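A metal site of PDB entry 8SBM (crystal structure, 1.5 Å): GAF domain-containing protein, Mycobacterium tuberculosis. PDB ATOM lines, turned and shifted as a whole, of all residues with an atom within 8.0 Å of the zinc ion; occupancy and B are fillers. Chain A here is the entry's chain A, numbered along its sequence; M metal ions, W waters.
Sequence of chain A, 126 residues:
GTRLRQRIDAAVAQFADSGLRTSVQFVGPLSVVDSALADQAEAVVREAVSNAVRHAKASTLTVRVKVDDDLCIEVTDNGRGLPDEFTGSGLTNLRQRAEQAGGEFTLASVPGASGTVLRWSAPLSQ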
ATOM      1  N   VAL A  65      -9.776  -3.964   2.187  1.00  0.00           N
ATOM      2  CA  VAL A  65      -8.378  -4.237   1.859  1.00  0.00           C
ATOM      3  C   VAL A  65      -8.303  -5.702   1.459  1.00  0.00           C
ATOM      4  O   VAL A  65      -8.646  -6.584   2.245  1.00  0.00           O
ATOM      5  CB  VAL A  65      -7.440  -3.950   3.039  1.00  0.00           C
ATOM      6  CG1 VAL A  65      -6.007  -4.332   2.681  1.00  0.00           C
ATOM      7  CG2 VAL A  65      -7.533  -2.495   3.448  1.00  0.00           C
ATOM      8  N   LYS A  66      -7.855  -5.950   0.230  1.00  0.00           N
ATOM      9  CA  LYS A  66      -7.859  -7.291  -0.331  1.00  0.00           C
ATOM     10  C   LYS A  66      -6.473  -7.638  -0.849  1.00  0.00           C
ATOM     11  O   LYS A  66      -5.810  -6.814  -1.495  1.00  0.00           O
ATOM     12  CB  LYS A  66      -8.894  -7.396  -1.453  1.00  0.00           C
ATOM     13  CG  LYS A  66      -8.965  -8.746  -2.140  1.00  0.00           C
ATOM     14  CD  LYS A  66     -10.270  -8.880  -2.933  1.00  0.00           C
ATOM     15  CE  LYS A  66     -10.479  -7.695  -3.861  1.00  0.00           C
ATOM     16  NZ  LYS A  66     -11.729  -7.817  -4.665  1.00  0.00           N
ATOM     17  N   VAL A  67      -6.020  -8.852  -0.549  1.00  0.00           N
ATOM     18  CA  VAL A  67      -4.788  -9.384  -1.112  1.00  0.00           C
ATOM     19  C   VAL A  67      -5.186 -10.571  -1.967  1.00  0.00           C
ATOM     20  O   VAL A  67      -5.654 -11.597  -1.451  1.00  0.00           O
ATOM     21  CB  VAL A  67      -3.792  -9.781  -0.020  1.00  0.00           C
ATOM     22  CG1 VAL A  67      -2.578 -10.482  -0.619  1.00  0.00           C
ATOM     23  CG2 VAL A  67      -3.366  -8.549   0.765  1.00  0.00           C
ATOM     24  N   ASP A  68      -5.041 -10.418  -3.286  1.00  0.00           N
ATOM     25  CA  ASP A  68      -5.351 -11.482  -4.228  1.00  0.00           C
ATOM     26  C   ASP A  68      -4.185 -11.648  -5.192  1.00  0.00           C
ATOM     27  O   ASP A  68      -3.093 -12.052  -4.792  1.00  0.00           O
ATOM     28  CB  ASP A  68      -6.671 -11.225  -4.957  1.00  0.00           C
ATOM     29  CG  ASP A  68      -6.956  -9.729  -5.188  1.00  0.00           C
ATOM     30  OD1 ASP A  68      -6.010  -8.911  -5.283  1.00  0.00           O
ATOM     31  OD2 ASP A  68      -8.142  -9.381  -5.286  1.00  0.00           O
ATOM     32  N   ASP A  69      -4.385 -11.306  -6.466  1.00  0.00           N
ATOM     33  CA  ASP A  69      -3.261 -11.226  -7.378  1.00  0.00           C
ATOM     34  C   ASP A  69      -2.342 -10.068  -7.010  1.00  0.00           C
ATOM     35  O   ASP A  69      -1.136 -10.109  -7.311  1.00  0.00           O
ATOM     36  CB  ASP A  69      -3.749 -11.079  -8.823  1.00  0.00           C
ATOM     37  CG  ASP A  69      -4.682  -9.897  -8.996  1.00  0.00           C
ATOM     38  OD1 ASP A  69      -5.754  -9.884  -8.370  1.00  0.00           O
ATOM     39  OD2 ASP A  69      -4.321  -8.975  -9.757  1.00  0.00           O
ATOM     40  N   ASP A  70      -2.891  -9.041  -6.372  1.00  0.00           N
ATOM     41  CA  ASP A  70      -2.141  -7.852  -5.967  1.00  0.00           C
ATOM     42  C   ASP A  70      -2.625  -7.437  -4.579  1.00  0.00           C
ATOM     43  O   ASP A  70      -3.332  -8.184  -3.902  1.00  0.00           O
ATOM     44  CB  ASP A  70      -2.324  -6.739  -7.011  1.00  0.00           C
ATOM     45  CG  ASP A  70      -3.783  -6.320  -7.177  1.00  0.00           C
ATOM     46  OD1 ASP A  70      -4.634  -6.739  -6.360  1.00  0.00           O
ATOM     47  OD2 ASP A  70      -4.085  -5.569  -8.130  1.00  0.00           O
ATOM     48  N   LEU A  71      -2.227  -6.247  -4.157  1.00  0.00           N
ATOM     49  CA  LEU A  71      -2.842  -5.582  -3.010  1.00  0.00           C
ATOM     50  C   LEU A  71      -3.782  -4.518  -3.542  1.00  0.00           C
ATOM     51  O   LEU A  71      -3.366  -3.663  -4.336  1.00  0.00           O
ATOM     52  CB  LEU A  71      -1.787  -4.926  -2.124  1.00  0.00           C
ATOM     53  CG  LEU A  71      -2.414  -4.021  -1.062  1.00  0.00           C
ATOM     54  CD1 LEU A  71      -3.121  -4.849  -0.003  1.00  0.00           C
ATOM     55  CD2 LEU A  71      -1.390  -3.097  -0.420  1.00  0.00           C
ATOM     56  N   CYS A  72      -5.039  -4.546  -3.121  1.00  0.00           N
ATOM     57  CA  CYS A  72      -5.971  -3.529  -3.571  1.00  0.00           C
ATOM     58  C   CYS A  72      -6.841  -3.037  -2.430  1.00  0.00           C
ATOM     59  O   CYS A  72      -7.345  -3.812  -1.608  1.00  0.00           O
ATOM     60  CB  CYS A  72      -6.821  -3.999  -4.772  1.00  0.00           C
ATOM     61  SG  CYS A  72      -7.741  -5.516  -4.522  1.00  0.00           S
ATOM     62  N   ILE A  73      -7.012  -1.721  -2.388  1.00  0.00           N
ATOM     63  CA  ILE A  73      -7.768  -1.014  -1.357  1.00  0.00           C
ATOM     64  C   ILE A  73      -8.925  -0.311  -2.054  1.00  0.00           C
ATOM     65  O   ILE A  73      -8.718   0.393  -3.047  1.00  0.00           O
ATOM     66  CB  ILE A  73      -6.880   0.028  -0.664  1.00  0.00           C
ATOM     67  CG1 ILE A  73      -5.657  -0.655  -0.058  1.00  0.00           C
ATOM     68  CG2 ILE A  73      -7.672   0.791   0.392  1.00  0.00           C
ATOM     69  CD1 ILE A  73      -4.608   0.291   0.382  1.00  0.00           C
ATOM     70  N   ARG A 119     -10.092   3.502  -5.501  1.00  0.00           N
ATOM     71  CA  ARG A 119      -9.459   2.204  -5.600  1.00  0.00           C
ATOM     72  C   ARG A 119      -7.969   2.415  -5.838  1.00  0.00           C
ATOM     73  O   ARG A 119      -7.576   3.130  -6.765  1.00  0.00           O
ATOM     74  CB  ARG A 119     -10.082   1.374  -6.736  1.00  0.00           C
ATOM     75  CG  ARG A 119      -9.887  -0.109  -6.610  1.00  0.00           C
ATOM     76  CD  ARG A 119     -10.517  -0.838  -7.791  1.00  0.00           C
ATOM     77  NE  ARG A 119     -11.792  -0.247  -8.172  1.00  0.00           N
ATOM     78  CZ  ARG A 119     -12.972  -0.623  -7.693  1.00  0.00           C
ATOM     79  NH1 ARG A 119     -13.073  -1.580  -6.784  1.00  0.00           N
ATOM     80  NH2 ARG A 119     -14.071  -0.013  -8.129  1.00  0.00           N
ATOM     81  N   TRP A 120      -7.151   1.822  -4.988  1.00  0.00           N
ATOM     82  CA  TRP A 120      -5.701   1.928  -5.080  1.00  0.00           C
ATOM     83  C   TRP A 120      -5.155   0.510  -5.076  1.00  0.00           C
ATOM     84  O   TRP A 120      -5.526  -0.287  -4.208  1.00  0.00           O
ATOM     85  CB  TRP A 120      -5.175   2.705  -3.863  1.00  0.00           C
ATOM     86  CG  TRP A 120      -3.733   3.119  -3.937  1.00  0.00           C
ATOM     87  CD1 TRP A 120      -3.262   4.345  -4.292  1.00  0.00           C
ATOM     88  CD2 TRP A 120      -2.583   2.318  -3.613  1.00  0.00           C
ATOM     89  NE1 TRP A 120      -1.886   4.353  -4.233  1.00  0.00           N
ATOM     90  CE2 TRP A 120      -1.447   3.126  -3.811  1.00  0.00           C
ATOM     91  CE3 TRP A 120      -2.412   1.002  -3.175  1.00  0.00           C
ATOM     92  CZ2 TRP A 120      -0.157   2.658  -3.601  1.00  0.00           C
ATOM     93  CZ3 TRP A 120      -1.122   0.534  -2.966  1.00  0.00           C
ATOM     94  CH2 TRP A 120      -0.015   1.368  -3.179  1.00  0.00           C
ATOM     95  N   SER A 121      -4.300   0.182  -6.034  1.00  0.00           N
ATOM     96  CA  SER A 121      -3.754  -1.162  -6.101  1.00  0.00           C
ATOM     97  C   SER A 121      -2.276  -1.100  -6.427  1.00  0.00           C
ATOM     98  O   SER A 121      -1.785  -0.128  -7.015  1.00  0.00           O
ATOM     99  CB  SER A 121      -4.499  -2.055  -7.108  1.00  0.00           C
ATOM    100  OG  SER A 121      -4.358  -1.575  -8.431  1.00  0.00           O
ATOM    101  N   ALA A 122      -1.557  -2.147  -6.031  1.00  0.00           N
ATOM    102  CA  ALA A 122      -0.143  -2.232  -6.338  1.00  0.00           C
ATOM    103  C   ALA A 122       0.242  -3.703  -6.420  1.00  0.00           C
ATOM    104  O   ALA A 122      -0.373  -4.536  -5.733  1.00  0.00           O
ATOM    105  CB  ALA A 122       0.709  -1.529  -5.268  1.00  0.00           C
ATOM    106  N   LEU A 124       2.226  -7.167  -5.742  1.00  0.00           N
ATOM    107  CA  LEU A 124       3.051  -7.780  -4.716  1.00  0.00           C
ATOM    108  C   LEU A 124       4.363  -8.216  -5.346  1.00  0.00           C
ATOM    109  O   LEU A 124       4.399  -8.665  -6.490  1.00  0.00           O
ATOM    110  CB  LEU A 124       2.341  -9.007  -4.147  1.00  0.00           C
ATOM    111  CG  LEU A 124       0.901  -8.799  -3.689  1.00  0.00           C
ATOM    112  CD1 LEU A 124       0.196 -10.135  -3.557  1.00  0.00           C
ATOM    113  CD2 LEU A 124       0.865  -8.051  -2.377  1.00  0.00           C
HETATM  114 ZN    ZN M   1      -6.557  -7.011  -5.879  1.00  0.00          ZN
HETATM  115  O   HOH W   1      -7.181  -7.369  -7.764  1.00  0.00           O
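O of Cys 72 sits at hydrogen-bond distance from N of Lys 66, 2.9 Å away.
The side-chain amino group (NZ) of Lys 66 lies within salt-bridge range of the side-chain carboxylate (OD2) of Asp 68 (3.96 Å).
Asp 69 touches the zinc ion (OD1 to ZN, 3.9 Å).
Of the 14 residues printed, 4 come within 4 Å of the zinc ion.
OD1 of Asp 70 binds the zinc ion.
Water W1 binds the zinc ion (2.0 Å).
The side-chain carboxylate (OD1) of Asp 68 binds the zinc ion.
SG of Cys 72 is bound to the zinc ion, 2.3 Å away.
Water W1 bridges the side-chain carboxylate (OD1) of Asp 69 (3.0 Å) and the side-chain carboxylate (OD2) of Asp 68 (3.3 Å).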
